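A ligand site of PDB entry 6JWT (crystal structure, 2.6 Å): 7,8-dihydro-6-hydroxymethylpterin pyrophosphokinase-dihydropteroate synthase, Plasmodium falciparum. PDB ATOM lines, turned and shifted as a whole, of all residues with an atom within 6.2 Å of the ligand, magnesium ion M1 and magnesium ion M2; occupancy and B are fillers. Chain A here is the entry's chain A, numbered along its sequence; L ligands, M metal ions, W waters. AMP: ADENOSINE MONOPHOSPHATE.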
ATOM      1  N   LEU A 181      14.005 -22.841  17.801  1.00  0.00           N
ATOM      2  CA  LEU A 181      13.895 -23.112  19.231  1.00  0.00           C
ATOM      3  C   LEU A 181      14.929 -24.151  19.674  1.00  0.00           C
ATOM      4  O   LEU A 181      15.581 -23.976  20.714  1.00  0.00           O
ATOM      5  CB  LEU A 181      12.459 -23.535  19.603  1.00  0.00           C
ATOM      6  CG  LEU A 181      12.123 -23.486  21.101  1.00  0.00           C
ATOM      7  CD1 LEU A 181      12.701 -22.244  21.774  1.00  0.00           C
ATOM      8  CD2 LEU A 181      10.629 -23.549  21.355  1.00  0.00           C
ATOM      9  N   LYS A 185      17.661 -23.435  22.472  1.00  0.00           N
ATOM     10  CA  LYS A 185      17.810 -24.252  23.656  1.00  0.00           C
ATOM     11  C   LYS A 185      19.265 -24.696  23.824  1.00  0.00           C
ATOM     12  O   LYS A 185      19.784 -24.723  24.930  1.00  0.00           O
ATOM     13  CB  LYS A 185      16.794 -25.398  23.663  1.00  0.00           C
ATOM     14  CG  LYS A 185      15.322 -24.984  23.676  1.00  0.00           C
ATOM     15  CD  LYS A 185      14.835 -24.398  24.997  1.00  0.00           C
ATOM     16  CE  LYS A 185      13.340 -24.180  25.045  1.00  0.00           C
ATOM     17  NZ  LYS A 185      12.921 -23.623  26.353  1.00  0.00           N
ATOM     18  N   GLU A 188      20.974 -21.722  25.124  1.00  0.00           N
ATOM     19  CA  GLU A 188      20.618 -21.550  26.523  1.00  0.00           C
ATOM     20  C   GLU A 188      21.471 -22.452  27.430  1.00  0.00           C
ATOM     21  O   GLU A 188      21.981 -22.006  28.468  1.00  0.00           O
ATOM     22  CB  GLU A 188      19.128 -21.761  26.762  1.00  0.00           C
ATOM     23  CG  GLU A 188      18.252 -20.726  26.081  1.00  0.00           C
ATOM     24  CD  GLU A 188      16.808 -20.810  26.542  1.00  0.00           C
ATOM     25  OE1 GLU A 188      16.573 -21.181  27.705  1.00  0.00           O
ATOM     26  OE2 GLU A 188      15.918 -20.513  25.721  1.00  0.00           O
ATOM     27  N   ASP A 208      16.567 -16.540  29.136  1.00  0.00           N
ATOM     28  CA  ASP A 208      15.345 -17.039  28.529  1.00  0.00           C
ATOM     29  C   ASP A 208      15.144 -16.328  27.182  1.00  0.00           C
ATOM     30  O   ASP A 208      14.690 -15.186  27.118  1.00  0.00           O
ATOM     31  CB  ASP A 208      14.163 -16.978  29.505  1.00  0.00           C
ATOM     32  CG  ASP A 208      12.784 -17.311  28.956  1.00  0.00           C
ATOM     33  OD1 ASP A 208      12.671 -18.273  28.159  1.00  0.00           O
ATOM     34  OD2 ASP A 208      11.807 -16.624  29.358  1.00  0.00           O
ATOM     35  N   ILE A 209      15.487 -17.032  26.098  1.00  0.00           N
ATOM     36  CA  ILE A 209      15.330 -16.510  24.747  1.00  0.00           C
ATOM     37  C   ILE A 209      14.058 -17.080  24.150  1.00  0.00           C
ATOM     38  O   ILE A 209      14.001 -18.253  23.802  1.00  0.00           O
ATOM     39  CB  ILE A 209      16.555 -16.864  23.876  1.00  0.00           C
ATOM     40  CG1 ILE A 209      17.865 -16.535  24.582  1.00  0.00           C
ATOM     41  CG2 ILE A 209      16.452 -16.231  22.503  1.00  0.00           C
ATOM     42  CD1 ILE A 209      19.113 -17.002  23.853  1.00  0.00           C
ATOM     43  N   ASP A 210      13.031 -16.239  24.015  1.00  0.00           N
ATOM     44  CA  ASP A 210      11.786 -16.710  23.417  1.00  0.00           C
ATOM     45  C   ASP A 210      11.732 -16.259  21.964  1.00  0.00           C
ATOM     46  O   ASP A 210      12.396 -15.299  21.596  1.00  0.00           O
ATOM     47  CB  ASP A 210      10.595 -16.168  24.205  1.00  0.00           C
ATOM     48  CG  ASP A 210      10.615 -16.638  25.645  1.00  0.00           C
ATOM     49  OD1 ASP A 210      11.166 -17.735  25.886  1.00  0.00           O
ATOM     50  OD2 ASP A 210      10.095 -15.901  26.501  1.00  0.00           O
ATOM     51  N   ILE A 211      10.936 -16.962  21.142  1.00  0.00           N
ATOM     52  CA  ILE A 211      10.647 -16.520  19.790  1.00  0.00           C
ATOM     53  C   ILE A 211       9.347 -15.731  19.832  1.00  0.00           C
ATOM     54  O   ILE A 211       8.298 -16.301  20.107  1.00  0.00           O
ATOM     55  CB  ILE A 211      10.537 -17.687  18.789  1.00  0.00           C
ATOM     56  CG1 ILE A 211      11.762 -18.612  18.873  1.00  0.00           C
ATOM     57  CG2 ILE A 211      10.268 -17.191  17.374  1.00  0.00           C
ATOM     58  CD1 ILE A 211      11.768 -19.729  17.850  1.00  0.00           C
ATOM     59  N   LEU A 212       9.426 -14.428  19.554  1.00  0.00           N
ATOM     60  CA  LEU A 212       8.207 -13.623  19.486  1.00  0.00           C
ATOM     61  C   LEU A 212       7.540 -13.851  18.142  1.00  0.00           C
ATOM     62  O   LEU A 212       6.383 -14.231  18.124  1.00  0.00           O
ATOM     63  CB  LEU A 212       8.485 -12.140  19.748  1.00  0.00           C
ATOM     64  CG  LEU A 212       9.105 -11.897  21.115  1.00  0.00           C
ATOM     65  CD1 LEU A 212       9.383 -10.424  21.325  1.00  0.00           C
ATOM     66  CD2 LEU A 212       8.218 -12.490  22.210  1.00  0.00           C
ATOM     67  N   ASP A 311      13.533 -32.559  27.033  1.00  0.00           N
ATOM     68  CA  ASP A 311      12.254 -32.311  27.687  1.00  0.00           C
ATOM     69  C   ASP A 311      11.877 -30.824  27.659  1.00  0.00           C
ATOM     70  O   ASP A 311      10.791 -30.464  28.098  1.00  0.00           O
ATOM     71  CB  ASP A 311      12.267 -32.812  29.140  1.00  0.00           C
ATOM     72  CG  ASP A 311      11.996 -34.302  29.305  1.00  0.00           C
ATOM     73  OD1 ASP A 311      11.223 -34.854  28.486  1.00  0.00           O
ATOM     74  OD2 ASP A 311      12.548 -34.896  30.249  1.00  0.00           O
ATOM     75  N   ASN A 312      12.769 -29.970  27.146  1.00  0.00           N
ATOM     76  CA  ASN A 312      12.650 -28.529  27.348  1.00  0.00           C
ATOM     77  C   ASN A 312      11.648 -27.901  26.368  1.00  0.00           C
ATOM     78  O   ASN A 312      11.129 -26.821  26.642  1.00  0.00           O
ATOM     79  CB  ASN A 312      14.023 -27.844  27.475  1.00  0.00           C
ATOM     80  CG  ASN A 312      14.835 -28.277  28.692  1.00  0.00           C
ATOM     81  OD1 ASN A 312      14.352 -29.008  29.554  1.00  0.00           O
ATOM     82  ND2 ASN A 312      16.076 -27.814  28.779  1.00  0.00           N
ATOM     83  N   ILE A 313      11.361 -28.571  25.228  1.00  0.00           N
ATOM     84  CA  ILE A 313      10.367 -28.115  24.270  1.00  0.00           C
ATOM     85  C   ILE A 313       9.096 -28.947  24.452  1.00  0.00           C
ATOM     86  O   ILE A 313       9.020 -30.089  24.017  1.00  0.00           O
ATOM     87  CB  ILE A 313      10.883 -28.241  22.823  1.00  0.00           C
ATOM     88  CG1 ILE A 313      12.310 -27.730  22.643  1.00  0.00           C
ATOM     89  CG2 ILE A 313       9.914 -27.613  21.812  1.00  0.00           C
ATOM     90  CD1 ILE A 313      12.981 -28.234  21.389  1.00  0.00           C
ATOM     91  N   GLU A 314       8.076 -28.337  25.085  1.00  0.00           N
ATOM     92  CA  GLU A 314       6.819 -29.029  25.332  1.00  0.00           C
ATOM     93  C   GLU A 314       5.849 -28.737  24.196  1.00  0.00           C
ATOM     94  O   GLU A 314       5.356 -29.672  23.567  1.00  0.00           O
ATOM     95  CB  GLU A 314       6.269 -28.679  26.730  1.00  0.00           C
ATOM     96  CG  GLU A 314       5.381 -29.762  27.347  1.00  0.00           C
ATOM     97  CD  GLU A 314       6.079 -30.898  28.075  1.00  0.00           C
ATOM     98  OE1 GLU A 314       6.939 -30.609  28.949  1.00  0.00           O
ATOM     99  OE2 GLU A 314       5.772 -32.072  27.777  1.00  0.00           O
ATOM    100  N   PHE A 315       5.581 -27.449  23.942  1.00  0.00           N
ATOM    101  CA  PHE A 315       4.789 -26.973  22.814  1.00  0.00           C
ATOM    102  C   PHE A 315       5.563 -25.881  22.053  1.00  0.00           C
ATOM    103  O   PHE A 315       6.753 -25.670  22.288  1.00  0.00           O
ATOM    104  CB  PHE A 315       3.429 -26.480  23.321  1.00  0.00           C
ATOM    105  CG  PHE A 315       3.454 -25.195  24.110  1.00  0.00           C
ATOM    106  CD1 PHE A 315       3.993 -25.165  25.382  1.00  0.00           C
ATOM    107  CD2 PHE A 315       2.933 -24.014  23.580  1.00  0.00           C
ATOM    108  CE1 PHE A 315       4.022 -23.983  26.119  1.00  0.00           C
ATOM    109  CE2 PHE A 315       2.940 -22.837  24.319  1.00  0.00           C
ATOM    110  CZ  PHE A 315       3.487 -22.826  25.585  1.00  0.00           C
ATOM    111  N   LEU A 316       4.875 -25.224  21.099  1.00  0.00           N
ATOM    112  CA  LEU A 316       5.411 -24.094  20.355  1.00  0.00           C
ATOM    113  C   LEU A 316       4.267 -23.190  19.927  1.00  0.00           C
ATOM    114  O   LEU A 316       3.458 -23.568  19.073  1.00  0.00           O
ATOM    115  CB  LEU A 316       6.217 -24.582  19.143  1.00  0.00           C
ATOM    116  CG  LEU A 316       6.767 -23.486  18.213  1.00  0.00           C
ATOM    117  CD1 LEU A 316       7.878 -22.694  18.894  1.00  0.00           C
ATOM    118  CD2 LEU A 316       7.286 -24.102  16.919  1.00  0.00           C
ATOM    119  N   SER A 317       4.253 -21.978  20.491  1.00  0.00           N
ATOM    120  CA  SER A 317       3.318 -20.918  20.152  1.00  0.00           C
ATOM    121  C   SER A 317       4.039 -19.804  19.398  1.00  0.00           C
ATOM    122  O   SER A 317       5.002 -19.242  19.914  1.00  0.00           O
ATOM    123  CB  SER A 317       2.714 -20.380  21.408  1.00  0.00           C
ATOM    124  OG  SER A 317       1.902 -19.265  21.113  1.00  0.00           O
ATOM    125  N   ILE A 318       3.584 -19.495  18.178  1.00  0.00           N
ATOM    126  CA  ILE A 318       3.982 -18.296  17.456  1.00  0.00           C
ATOM    127  C   ILE A 318       2.717 -17.584  17.021  1.00  0.00           C
ATOM    128  O   ILE A 318       1.937 -18.174  16.279  1.00  0.00           O
ATOM    129  CB  ILE A 318       4.877 -18.594  16.216  1.00  0.00           C
ATOM    130  CG1 ILE A 318       6.208 -19.296  16.525  1.00  0.00           C
ATOM    131  CG2 ILE A 318       5.072 -17.336  15.372  1.00  0.00           C
ATOM    132  CD1 ILE A 318       6.975 -18.728  17.698  1.00  0.00           C
ATOM    133  N   PRO A 319       2.470 -16.299  17.417  1.00  0.00           N
ATOM    134  CA  PRO A 319       3.325 -15.544  18.334  1.00  0.00           C
ATOM    135  C   PRO A 319       3.449 -16.159  19.725  1.00  0.00           C
ATOM    136  O   PRO A 319       2.603 -16.966  20.110  1.00  0.00           O
ATOM    137  CB  PRO A 319       2.548 -14.245  18.511  1.00  0.00           C
ATOM    138  CG  PRO A 319       1.848 -14.061  17.182  1.00  0.00           C
ATOM    139  CD  PRO A 319       1.385 -15.470  16.857  1.00  0.00           C
ATOM    140  N   HIS A 320       4.483 -15.756  20.461  1.00  0.00           N
ATOM    141  CA  HIS A 320       4.678 -16.227  21.822  1.00  0.00           C
ATOM    142  C   HIS A 320       3.470 -15.813  22.660  1.00  0.00           C
ATOM    143  O   HIS A 320       2.805 -14.824  22.364  1.00  0.00           O
ATOM    144  CB  HIS A 320       6.012 -15.709  22.353  1.00  0.00           C
ATOM    145  CG  HIS A 320       6.451 -16.242  23.668  1.00  0.00           C
ATOM    146  ND1 HIS A 320       5.950 -15.756  24.864  1.00  0.00           N
ATOM    147  CD2 HIS A 320       7.410 -17.142  23.999  1.00  0.00           C
ATOM    148  CE1 HIS A 320       6.553 -16.355  25.884  1.00  0.00           C
ATOM    149  NE2 HIS A 320       7.445 -17.218  25.369  1.00  0.00           N
ATOM    150  N   VAL A 321       3.151 -16.626  23.675  1.00  0.00           N
ATOM    151  CA  VAL A 321       1.863 -16.508  24.362  1.00  0.00           C
ATOM    152  C   VAL A 321       1.725 -15.090  24.896  1.00  0.00           C
ATOM    153  O   VAL A 321       0.702 -14.439  24.686  1.00  0.00           O
ATOM    154  CB  VAL A 321       1.750 -17.583  25.468  1.00  0.00           C
ATOM    155  CG1 VAL A 321       0.517 -17.388  26.332  1.00  0.00           C
ATOM    156  CG2 VAL A 321       1.778 -18.982  24.888  1.00  0.00           C
ATOM    157  N   TYR A 322       2.812 -14.596  25.513  1.00  0.00           N
ATOM    158  CA  TYR A 322       2.763 -13.395  26.325  1.00  0.00           C
ATOM    159  C   TYR A 322       2.960 -12.095  25.532  1.00  0.00           C
ATOM    160  O   TYR A 322       2.895 -11.014  26.122  1.00  0.00           O
ATOM    161  CB  TYR A 322       3.701 -13.536  27.518  1.00  0.00           C
ATOM    162  CG  TYR A 322       3.132 -14.469  28.552  1.00  0.00           C
ATOM    163  CD1 TYR A 322       2.130 -14.038  29.419  1.00  0.00           C
ATOM    164  CD2 TYR A 322       3.532 -15.786  28.625  1.00  0.00           C
ATOM    165  CE1 TYR A 322       1.568 -14.897  30.350  1.00  0.00           C
ATOM    166  CE2 TYR A 322       2.987 -16.663  29.555  1.00  0.00           C
ATOM    167  CZ  TYR A 322       2.003 -16.209  30.415  1.00  0.00           C
ATOM    168  OH  TYR A 322       1.452 -17.057  31.339  1.00  0.00           O
ATOM    169  N   ARG A 326       2.587  -9.081  28.332  1.00  0.00           N
ATOM    170  CA  ARG A 326       3.699  -8.603  29.157  1.00  0.00           C
ATOM    171  C   ARG A 326       4.101  -7.194  28.707  1.00  0.00           C
ATOM    172  O   ARG A 326       4.262  -6.958  27.519  1.00  0.00           O
ATOM    173  CB  ARG A 326       4.892  -9.564  29.091  1.00  0.00           C
ATOM    174  CG  ARG A 326       5.115 -10.393  30.351  1.00  0.00           C
ATOM    175  CD  ARG A 326       6.436 -11.148  30.346  1.00  0.00           C
ATOM    176  NE  ARG A 326       6.557 -12.177  31.381  1.00  0.00           N
ATOM    177  CZ  ARG A 326       6.234 -13.469  31.242  1.00  0.00           C
ATOM    178  NH1 ARG A 326       5.755 -13.920  30.097  1.00  0.00           N
ATOM    179  NH2 ARG A 326       6.389 -14.299  32.246  1.00  0.00           N
HETATM  180  P   AMP L   1       7.780 -19.928  27.886  1.00  0.00           P
HETATM  181  O1P AMP L   1       8.698 -19.025  27.063  1.00  0.00           O
HETATM  182  O2P AMP L   1       6.461 -20.227  27.184  1.00  0.00           O
HETATM  183  O3P AMP L   1       7.604 -19.439  29.334  1.00  0.00           O
HETATM  184  O5' AMP L   1       8.609 -21.334  28.003  1.00  0.00           O
HETATM  185  C5' AMP L   1       7.956 -22.485  28.604  1.00  0.00           C
HETATM  186  C4' AMP L   1       7.709 -23.553  27.569  1.00  0.00           C
HETATM  187  O4' AMP L   1       7.025 -22.988  26.411  1.00  0.00           O
HETATM  188  C3' AMP L   1       8.962 -24.266  27.010  1.00  0.00           C
HETATM  189  O3' AMP L   1       8.741 -25.667  26.947  1.00  0.00           O
HETATM  190  C2' AMP L   1       9.094 -23.683  25.609  1.00  0.00           C
HETATM  191  O2' AMP L   1       9.743 -24.592  24.748  1.00  0.00           O
HETATM  192  C1' AMP L   1       7.637 -23.467  25.237  1.00  0.00           C
HETATM  193  N9  AMP L   1       7.386 -22.519  24.137  1.00  0.00           N
HETATM  194  C8  AMP L   1       6.248 -22.481  23.374  1.00  0.00           C
HETATM  195  N7  AMP L   1       6.268 -21.556  22.452  1.00  0.00           N
HETATM  196  C5  AMP L   1       7.501 -20.948  22.596  1.00  0.00           C
HETATM  197  C6  AMP L   1       8.124 -19.883  21.905  1.00  0.00           C
HETATM  198  N6  AMP L   1       7.559 -19.233  20.895  1.00  0.00           N
HETATM  199  N1  AMP L   1       9.366 -19.516  22.296  1.00  0.00           N
HETATM  200  C2  AMP L   1       9.934 -20.171  23.330  1.00  0.00           C
HETATM  201  N3  AMP L   1       9.436 -21.173  24.054  1.00  0.00           N
HETATM  202  C4  AMP L   1       8.204 -21.533  23.633  1.00  0.00           C
HETATM  203 MG    MG M   1      10.569 -18.428  27.957  1.00  0.00          MG
HETATM  204 MG    MG M   2       9.118 -19.806  30.723  1.00  0.00          MG
HETATM  205  O   HOH W   1       9.309 -16.798  28.844  1.00  0.00           O
HETATM  206  O   HOH W   2      10.896 -21.028  29.828  1.00  0.00           O
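Magnesium ion M2 is bound by an oxygen (O3P) of the ligand, at 2.1 Å. Magnesium ion M2 is bound by water W2 (2.3 Å).
NE2 of His 320 lies close to O1P of the ligand (2.8 Å). A nitrogen (N7) of the ligand lies within hydrogen-bond range of the backbone NH of Ser 317, 2.8 Å away. A nitrogen (N6) of the ligand is in hydrogen-bond range of the backbone carbonyl oxygen (O) of Ile 211 (3.1 Å). An oxygen (O3') of the ligand is in hydrogen-bond range of the backbone carbonyl oxygen (O) of Asn 312. An oxygen (O3') of the ligand is in hydrogen-bond range of the backbone NH of Glu 314 (3.3 Å). A nitrogen (N1) of the ligand lies within hydrogen-bond range of the backbone NH of Ile 211 (3.2 Å). The backbone carbonyl oxygen (O) of Ser 317 lies within hydrogen-bond range of a nitrogen (N6) of the ligand (2.7 Å).
A ring nitrogen (ND1) of His 320 sits close to the backbone NH (N) of Tyr 322 (3.4 Å). OD2 of Asp 210 lies within hydrogen-bond range of NE2 of His 320, 3.2 Å away. The backbone NH (N) of His 320 lies within hydrogen-bond range of the backbone carbonyl oxygen (O) of Leu 212. The backbone carbonyl oxygen (O) of Pro 319 lies within hydrogen-bond range of the side-chain hydroxyl (OG) of Ser 317 (2.6 Å).
CD2 of Leu 181 touches O2' of the ligand, at 3.7 Å. CE of Lys 185 touches O2' of the ligand (3.6 Å). Ile 313 touches the ligand (CA to O2', 3.6 Å). CE1 of Phe 315 touches O4' of the ligand (3.2 Å). Leu 316 touches the ligand. Ile 318 touches the ligand (CD1 to N6, 3.3 Å). Hydrophobic or aromatic side chains that line the ligand: Leu 181, Ile 211, Phe 315, Ile 318 and His 320. Within 4 Å of the ligand: Leu 181, Lys 185, Asp 210, Ile 211, Asn 312, Ile 313, Glu 314, Phe 315, Leu 316, Ser 317, Ile 318 and His 320. The nearest printed residue that does not touch the ligand is Asp 208 (4.2 Å).
No residue comes within 4 Å of magnesium ion M2. The nearest printed residue that does not touch magnesium ion M2 is Asp 208 (4.4 Å).
Magnesium ion M1 is bound by OD1 of Asp 208 (2.1 Å), O1P of the ligand (2.2 Å), water W1 (2.2 Å), OD1 of Asp 210 (2.3 Å) and OD2 of Asp 208 (2.6 Å). Magnesium ion M1 has five donor atoms within binding distance.
Two residues have an atom within 4 Å of magnesium ion M1: Asp 208 and Asp 210.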
